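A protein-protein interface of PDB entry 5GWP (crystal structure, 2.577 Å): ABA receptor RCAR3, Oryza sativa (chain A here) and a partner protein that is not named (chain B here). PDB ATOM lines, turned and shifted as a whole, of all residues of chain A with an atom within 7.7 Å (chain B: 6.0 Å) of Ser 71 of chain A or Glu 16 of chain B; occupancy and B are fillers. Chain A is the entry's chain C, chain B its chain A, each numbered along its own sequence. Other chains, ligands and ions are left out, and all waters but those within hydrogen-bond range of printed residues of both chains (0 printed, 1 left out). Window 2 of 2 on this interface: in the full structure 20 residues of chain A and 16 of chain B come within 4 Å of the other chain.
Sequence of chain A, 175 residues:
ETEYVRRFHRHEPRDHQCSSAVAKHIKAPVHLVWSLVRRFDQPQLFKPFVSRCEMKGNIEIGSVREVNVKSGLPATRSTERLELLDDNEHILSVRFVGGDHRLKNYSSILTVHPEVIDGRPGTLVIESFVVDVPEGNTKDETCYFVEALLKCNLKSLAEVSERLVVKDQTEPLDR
The side-chain hydroxyl (OG) of Ser 71 of chain A lies within hydrogen-bond range of the side-chain carboxylate (OE1) of Glu 16 of chain B. N of Gly 63 of chain B sits at hydrogen-bond distance from OG of Ser 71 of chain A (2.9 Å).
The backbone NH (N) of Gly 61 of chain B is in hydrogen-bond range of the backbone carbonyl oxygen (O) of Glu 16 of chain B, at 2.8 Å. The side-chain carboxylate (OE2) of Glu 16 of chain B lies within hydrogen-bond range of the backbone NH (N) of Gly 64 of chain B (3.0 Å). The side-chain amide oxygen (OD1) of Asn 311 of chain B lies within hydrogen-bond range of the backbone NH (N) of Glu 16 of chain B (3.0 Å). N of Lys 70 of chain A lies within hydrogen-bond range of O of Phe 49 of chain A (2.7 Å).
Among the printed residues, pairs that only touch across the chains: Ser 71 of chain A with His 62 of chain B (3.4 Å), Phe 49 of chain A with Asn 140 of chain B (3.7 Å) and Lys 70 of chain A with Gly 63 of chain B (3.9 Å).
Of chain B, only Glu 16 (2.6 Å), His 62 (3.4 Å) and Gly 63 (2.9 Å) come within 4 Å of Ser 71 of chain A. Printed residues of chain A within 4 Å of Glu 16 of chain B: Ser 71 (2.6 Å). No residue of chain A comes within 4 Å of Gly 64 of chain B. Of the printed residues of chain A, Gly 63 of chain B touches Lys 70 and Ser 71. Printed residues of chain B within 4 Å of Lys 70 of chain A: Gly 63. Of the printed residues of chain A, His 62 of chain B touches Ser 71. Of the printed residues of chain A, Asn 140 of chain B touches Phe 49. Printed residues of chain B within 4 Å of Phe 49 of chain A: Asn 140. Ser 51 of chain A touches none of the printed residues of chain B. Ala 75 of chain A touches none of the printed residues of chain B. The nearest residue of chain A that does not touch Glu 16 of chain B is Lys 70 of chain A (5.7 Å). The nearest printed residue of chain A that does not touch His 62 of chain B is Gly 72 of chain A (4.2 Å).
Hydrophobic or aromatic side chains of chain B that line the printed part of chain A: His 62. Among the printed residues, 5 pairs touch across the chains. Among the printed residues, no Asp or Glu carboxylate lies within 4 Å of a Lys or Arg side-chain nitrogen of the other chain.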
ATOM      1  N   PHE A  49      28.426 -20.000  21.559  1.00  0.00           N
ATOM      2  CA  PHE A  49      27.247 -19.230  21.199  1.00  0.00           C
ATOM      3  C   PHE A  49      26.024 -19.575  22.034  1.00  0.00           C
ATOM      4  O   PHE A  49      25.017 -18.869  21.941  1.00  0.00           O
ATOM      5  CB  PHE A  49      26.922 -19.416  19.713  1.00  0.00           C
ATOM      6  CG  PHE A  49      28.045 -19.032  18.795  1.00  0.00           C
ATOM      7  CD1 PHE A  49      28.319 -17.699  18.539  1.00  0.00           C
ATOM      8  CD2 PHE A  49      28.823 -20.000  18.182  1.00  0.00           C
ATOM      9  CE1 PHE A  49      29.352 -17.338  17.696  1.00  0.00           C
ATOM     10  CE2 PHE A  49      29.856 -19.646  17.336  1.00  0.00           C
ATOM     11  CZ  PHE A  49      30.120 -18.313  17.094  1.00  0.00           C
ATOM     12  N   SER A  51      23.782 -19.615  25.212  1.00  0.00           N
ATOM     13  CA  SER A  51      23.549 -18.907  26.465  1.00  0.00           C
ATOM     14  C   SER A  51      22.694 -19.701  27.441  1.00  0.00           C
ATOM     15  O   SER A  51      22.938 -19.648  28.650  1.00  0.00           O
ATOM     16  CB  SER A  51      22.887 -17.550  26.192  1.00  0.00           C
ATOM     17  OG  SER A  51      21.645 -17.704  25.526  1.00  0.00           O
ATOM     18  N   ASN A  68      18.986 -21.569  23.488  1.00  0.00           N
ATOM     19  CA  ASN A  68      18.975 -20.137  23.231  1.00  0.00           C
ATOM     20  C   ASN A  68      20.409 -19.684  23.004  1.00  0.00           C
ATOM     21  O   ASN A  68      21.293 -19.992  23.809  1.00  0.00           O
ATOM     22  CB  ASN A  68      18.352 -19.368  24.398  1.00  0.00           C
ATOM     23  CG  ASN A  68      16.889 -19.703  24.604  1.00  0.00           C
ATOM     24  OD1 ASN A  68      16.552 -20.652  25.311  1.00  0.00           O
ATOM     25  ND2 ASN A  68      16.011 -18.923  23.986  1.00  0.00           N
ATOM     26  N   VAL A  69      20.644 -18.975  21.906  1.00  0.00           N
ATOM     27  CA  VAL A  69      21.979 -18.548  21.545  1.00  0.00           C
ATOM     28  C   VAL A  69      22.171 -17.085  21.929  1.00  0.00           C
ATOM     29  O   VAL A  69      21.219 -16.356  22.196  1.00  0.00           O
ATOM     30  CB  VAL A  69      22.276 -18.777  20.044  1.00  0.00           C
ATOM     31  CG1 VAL A  69      22.089 -20.241  19.679  1.00  0.00           C
ATOM     32  CG2 VAL A  69      21.406 -17.884  19.189  1.00  0.00           C
ATOM     33  N   LYS A  70      23.428 -16.647  21.944  1.00  0.00           N
ATOM     34  CA  LYS A  70      23.778 -15.304  22.373  1.00  0.00           C
ATOM     35  C   LYS A  70      23.472 -14.290  21.272  1.00  0.00           C
ATOM     36  O   LYS A  70      22.909 -14.614  20.223  1.00  0.00           O
ATOM     37  CB  LYS A  70      25.251 -15.246  22.776  1.00  0.00           C
ATOM     38  CG  LYS A  70      25.640 -16.211  23.885  1.00  0.00           C
ATOM     39  CD  LYS A  70      26.951 -15.786  24.525  1.00  0.00           C
ATOM     40  CE  LYS A  70      27.387 -16.754  25.612  1.00  0.00           C
ATOM     41  NZ  LYS A  70      28.101 -17.928  25.041  1.00  0.00           N
ATOM     42  N   SER A  71      23.845 -13.038  21.521  1.00  0.00           N
ATOM     43  CA  SER A  71      23.599 -11.957  20.581  1.00  0.00           C
ATOM     44  C   SER A  71      24.662 -11.937  19.486  1.00  0.00           C
ATOM     45  O   SER A  71      25.739 -12.527  19.614  1.00  0.00           O
ATOM     46  CB  SER A  71      23.573 -10.613  21.306  1.00  0.00           C
ATOM     47  OG  SER A  71      24.833 -10.333  21.889  1.00  0.00           O
ATOM     48  N   GLY A  72      24.345 -11.239  18.396  1.00  0.00           N
ATOM     49  CA  GLY A  72      25.257 -11.159  17.273  1.00  0.00           C
ATOM     50  C   GLY A  72      25.172 -12.313  16.304  1.00  0.00           C
ATOM     51  O   GLY A  72      26.130 -12.556  15.563  1.00  0.00           O
ATOM     52  N   LEU A  73      24.060 -13.037  16.287  1.00  0.00           N
ATOM     53  CA  LEU A  73      23.888 -14.231  15.479  1.00  0.00           C
ATOM     54  C   LEU A  73      22.655 -14.106  14.590  1.00  0.00           C
ATOM     55  O   LEU A  73      21.762 -13.297  14.864  1.00  0.00           O
ATOM     56  CB  LEU A  73      23.762 -15.467  16.383  1.00  0.00           C
ATOM     57  CG  LEU A  73      25.062 -15.879  17.079  1.00  0.00           C
ATOM     58  CD1 LEU A  73      24.799 -16.942  18.133  1.00  0.00           C
ATOM     59  CD2 LEU A  73      26.079 -16.370  16.060  1.00  0.00           C
ATOM     60  N   PRO A  74      22.577 -14.892  13.509  1.00  0.00           N
ATOM     61  CA  PRO A  74      21.398 -14.827  12.630  1.00  0.00           C
ATOM     62  C   PRO A  74      20.140 -15.429  13.231  1.00  0.00           C
ATOM     63  O   PRO A  74      19.077 -15.342  12.603  1.00  0.00           O
ATOM     64  CB  PRO A  74      21.835 -15.624  11.388  1.00  0.00           C
ATOM     65  CG  PRO A  74      23.308 -15.802  11.513  1.00  0.00           C
ATOM     66  CD  PRO A  74      23.620 -15.777  12.966  1.00  0.00           C
ATOM     67  N   ALA A  75      20.217 -16.037  14.413  1.00  0.00           N
ATOM     68  CA  ALA A  75      19.070 -16.682  15.034  1.00  0.00           C
ATOM     69  C   ALA A  75      19.152 -16.483  16.539  1.00  0.00           C
ATOM     70  O   ALA A  75      20.120 -15.920  17.060  1.00  0.00           O
ATOM     71  CB  ALA A  75      19.008 -18.170  14.673  1.00  0.00           C
ATOM     72  N   THR A  76      18.120 -16.941  17.240  1.00  0.00           N
ATOM     73  CA  THR A  76      18.043 -16.824  18.691  1.00  0.00           C
ATOM     74  C   THR A  76      17.862 -18.159  19.395  1.00  0.00           C
ATOM     75  O   THR A  76      18.438 -18.369  20.465  1.00  0.00           O
ATOM     76  CB  THR A  76      16.892 -15.885  19.093  1.00  0.00           C
ATOM     77  OG1 THR A  76      15.662 -16.369  18.543  1.00  0.00           O
ATOM     78  CG2 THR A  76      17.151 -14.475  18.582  1.00  0.00           C
ATOM     79  N   GLU B  14      19.823  -9.356  28.608  1.00  0.00           N
ATOM     80  CA  GLU B  14      21.110  -8.902  29.105  1.00  0.00           C
ATOM     81  C   GLU B  14      21.429  -7.509  28.578  1.00  0.00           C
ATOM     82  O   GLU B  14      20.908  -7.074  27.547  1.00  0.00           O
ATOM     83  CB  GLU B  14      22.219  -9.875  28.692  1.00  0.00           C
ATOM     84  CG  GLU B  14      22.063 -11.270  29.267  1.00  0.00           C
ATOM     85  CD  GLU B  14      22.795 -12.319  28.455  1.00  0.00           C
ATOM     86  OE1 GLU B  14      22.400 -12.556  27.294  1.00  0.00           O
ATOM     87  OE2 GLU B  14      23.780 -12.892  28.969  1.00  0.00           O
ATOM     88  N   MET B  15      22.298  -6.812  29.305  1.00  0.00           N
ATOM     89  CA  MET B  15      22.779  -5.494  28.913  1.00  0.00           C
ATOM     90  C   MET B  15      24.198  -5.630  28.379  1.00  0.00           C
ATOM     91  O   MET B  15      25.112  -5.998  29.123  1.00  0.00           O
ATOM     92  CB  MET B  15      22.738  -4.518  30.089  1.00  0.00           C
ATOM     93  CG  MET B  15      23.171  -3.102  29.730  1.00  0.00           C
ATOM     94  SD  MET B  15      22.251  -2.408  28.340  1.00  0.00           S
ATOM     95  CE  MET B  15      22.647  -0.670  28.507  1.00  0.00           C
ATOM     96  N   GLU B  16      24.380  -5.330  27.094  1.00  0.00           N
ATOM     97  CA  GLU B  16      25.698  -5.380  26.475  1.00  0.00           C
ATOM     98  C   GLU B  16      26.093  -4.052  25.843  1.00  0.00           C
ATOM     99  O   GLU B  16      27.107  -3.988  25.137  1.00  0.00           O
ATOM    100  CB  GLU B  16      25.746  -6.509  25.441  1.00  0.00           C
ATOM    101  CG  GLU B  16      25.637  -7.896  26.066  1.00  0.00           C
ATOM    102  CD  GLU B  16      25.467  -8.999  25.039  1.00  0.00           C
ATOM    103  OE1 GLU B  16      25.328  -8.682  23.839  1.00  0.00           O
ATOM    104  OE2 GLU B  16      25.469 -10.184  25.434  1.00  0.00           O
ATOM    105  N   ASP B  17      25.327  -2.992  26.081  1.00  0.00           N
ATOM    106  CA  ASP B  17      25.696  -1.655  25.644  1.00  0.00           C
ATOM    107  C   ASP B  17      26.458  -0.942  26.752  1.00  0.00           C
ATOM    108  O   ASP B  17      26.182  -1.138  27.940  1.00  0.00           O
ATOM    109  CB  ASP B  17      24.458  -0.846  25.256  1.00  0.00           C
ATOM    110  CG  ASP B  17      24.080  -1.017  23.797  1.00  0.00           C
ATOM    111  OD1 ASP B  17      24.545  -1.993  23.175  1.00  0.00           O
ATOM    112  OD2 ASP B  17      23.317  -0.178  23.274  1.00  0.00           O
ATOM    113  N   ALA B  18      27.426  -0.122  26.354  1.00  0.00           N
ATOM    114  CA  ALA B  18      28.184   0.701  27.283  1.00  0.00           C
ATOM    115  C   ALA B  18      28.429   2.058  26.640  1.00  0.00           C
ATOM    116  O   ALA B  18      28.345   2.213  25.420  1.00  0.00           O
ATOM    117  CB  ALA B  18      29.512   0.042  27.679  1.00  0.00           C
ATOM    118  N   PHE B  59      29.344   1.995  22.733  1.00  0.00           N
ATOM    119  CA  PHE B  59      29.945   0.691  22.471  1.00  0.00           C
ATOM    120  C   PHE B  59      28.861  -0.372  22.572  1.00  0.00           C
ATOM    121  O   PHE B  59      28.391  -0.682  23.671  1.00  0.00           O
ATOM    122  CB  PHE B  59      31.086   0.405  23.448  1.00  0.00           C
ATOM    123  CG  PHE B  59      32.002   1.574  23.665  1.00  0.00           C
ATOM    124  CD1 PHE B  59      33.007   1.861  22.757  1.00  0.00           C
ATOM    125  CD2 PHE B  59      31.850   2.394  24.770  1.00  0.00           C
ATOM    126  CE1 PHE B  59      33.848   2.938  22.951  1.00  0.00           C
ATOM    127  CE2 PHE B  59      32.687   3.474  24.968  1.00  0.00           C
ATOM    128  CZ  PHE B  59      33.689   3.746  24.059  1.00  0.00           C
ATOM    129  N   ASP B  60      28.465  -0.928  21.429  1.00  0.00           N
ATOM    130  CA  ASP B  60      27.407  -1.932  21.354  1.00  0.00           C
ATOM    131  C   ASP B  60      28.068  -3.305  21.350  1.00  0.00           C
ATOM    132  O   ASP B  60      28.558  -3.770  20.316  1.00  0.00           O
ATOM    133  CB  ASP B  60      26.548  -1.716  20.112  1.00  0.00           C
ATOM    134  CG  ASP B  60      25.313  -2.600  20.085  1.00  0.00           C
ATOM    135  OD1 ASP B  60      25.204  -3.519  20.923  1.00  0.00           O
ATOM    136  OD2 ASP B  60      24.447  -2.377  19.214  1.00  0.00           O
ATOM    137  N   GLY B  61      28.082  -3.957  22.513  1.00  0.00           N
ATOM    138  CA  GLY B  61      28.692  -5.262  22.613  1.00  0.00           C
ATOM    139  C   GLY B  61      27.794  -6.373  22.102  1.00  0.00           C
ATOM    140  O   GLY B  61      26.569  -6.265  22.081  1.00  0.00           O
ATOM    141  N   HIS B  62      28.431  -7.464  21.687  1.00  0.00           N
ATOM    142  CA  HIS B  62      27.725  -8.661  21.257  1.00  0.00           C
ATOM    143  C   HIS B  62      28.456  -9.887  21.781  1.00  0.00           C
ATOM    144  O   HIS B  62      29.672  -9.863  21.986  1.00  0.00           O
ATOM    145  CB  HIS B  62      27.600  -8.721  19.729  1.00  0.00           C
ATOM    146  CG  HIS B  62      28.874  -8.414  19.005  1.00  0.00           C
ATOM    147  ND1 HIS B  62      29.193  -7.145  18.571  1.00  0.00           N
ATOM    148  CD2 HIS B  62      29.906  -9.209  18.638  1.00  0.00           C
ATOM    149  CE1 HIS B  62      30.367  -7.172  17.969  1.00  0.00           C
ATOM    150  NE2 HIS B  62      30.822  -8.412  17.995  1.00  0.00           N
ATOM    151  N   GLY B  63      27.700 -10.961  22.003  1.00  0.00           N
ATOM    152  CA  GLY B  63      28.264 -12.138  22.631  1.00  0.00           C
ATOM    153  C   GLY B  63      28.696 -11.941  24.066  1.00  0.00           C
ATOM    154  O   GLY B  63      29.397 -12.798  24.612  1.00  0.00           O
ATOM    155  N   GLY B  64      28.288 -10.840  24.694  1.00  0.00           N
ATOM    156  CA  GLY B  64      28.726 -10.485  26.028  1.00  0.00           C
ATOM    157  C   GLY B  64      29.001  -9.000  26.135  1.00  0.00           C
ATOM    158  O   GLY B  64      29.026  -8.296  25.121  1.00  0.00           O
ATOM    159  N   ALA B  65      29.213  -8.504  27.353  1.00  0.00           N
ATOM    160  CA  ALA B  65      29.431  -7.082  27.582  1.00  0.00           C
ATOM    161  C   ALA B  65      30.867  -6.736  27.947  1.00  0.00           C
ATOM    162  O   ALA B  65      31.167  -5.557  28.157  1.00  0.00           O
ATOM    163  CB  ALA B  65      28.484  -6.576  28.679  1.00  0.00           C
ATOM    164  N   ALA B  68      32.759  -4.283  25.374  1.00  0.00           N
ATOM    165  CA  ALA B  68      32.214  -2.928  25.403  1.00  0.00           C
ATOM    166  C   ALA B  68      32.663  -2.184  26.655  1.00  0.00           C
ATOM    167  O   ALA B  68      33.132  -1.039  26.581  1.00  0.00           O
ATOM    168  CB  ALA B  68      30.688  -2.975  25.320  1.00  0.00           C
ATOM    169  N   ASN B 140      34.566 -15.004  20.649  1.00  0.00           N
ATOM    170  CA  ASN B 140      33.348 -14.620  19.947  1.00  0.00           C
ATOM    171  C   ASN B 140      32.672 -13.406  20.570  1.00  0.00           C
ATOM    172  O   ASN B 140      31.506 -13.132  20.265  1.00  0.00           O
ATOM    173  CB  ASN B 140      32.367 -15.795  19.898  1.00  0.00           C
ATOM    174  CG  ASN B 140      31.804 -16.144  21.260  1.00  0.00           C
ATOM    175  OD1 ASN B 140      32.454 -15.944  22.285  1.00  0.00           O
ATOM    176  ND2 ASN B 140      30.581 -16.662  21.279  1.00  0.00           N
ATOM    177  N   SER B 143      32.576  -5.745  20.211  1.00  0.00           N
ATOM    178  CA  SER B 143      31.815  -4.534  20.480  1.00  0.00           C
ATOM    179  C   SER B 143      32.065  -3.518  19.376  1.00  0.00           C
ATOM    180  O   SER B 143      33.175  -3.429  18.843  1.00  0.00           O
ATOM    181  CB  SER B 143      32.190  -3.936  21.840  1.00  0.00           C
ATOM    182  OG  SER B 143      31.423  -2.779  22.125  1.00  0.00           O
ATOM    183  N   ASN B 311      19.012  -3.364  23.303  1.00  0.00           N
ATOM    184  CA  ASN B 311      19.597  -2.387  24.211  1.00  0.00           C
ATOM    185  C   ASN B 311      19.677  -1.037  23.513  1.00  0.00           C
ATOM    186  O   ASN B 311      19.966  -0.960  22.315  1.00  0.00           O
ATOM    187  CB  ASN B 311      20.993  -2.829  24.656  1.00  0.00           C
ATOM    188  CG  ASN B 311      20.989  -4.177  25.346  1.00  0.00           C
ATOM    189  OD1 ASN B 311      22.007  -4.868  25.382  1.00  0.00           O
ATOM    190  ND2 ASN B 311      19.845  -4.558  25.902  1.00  0.00           N
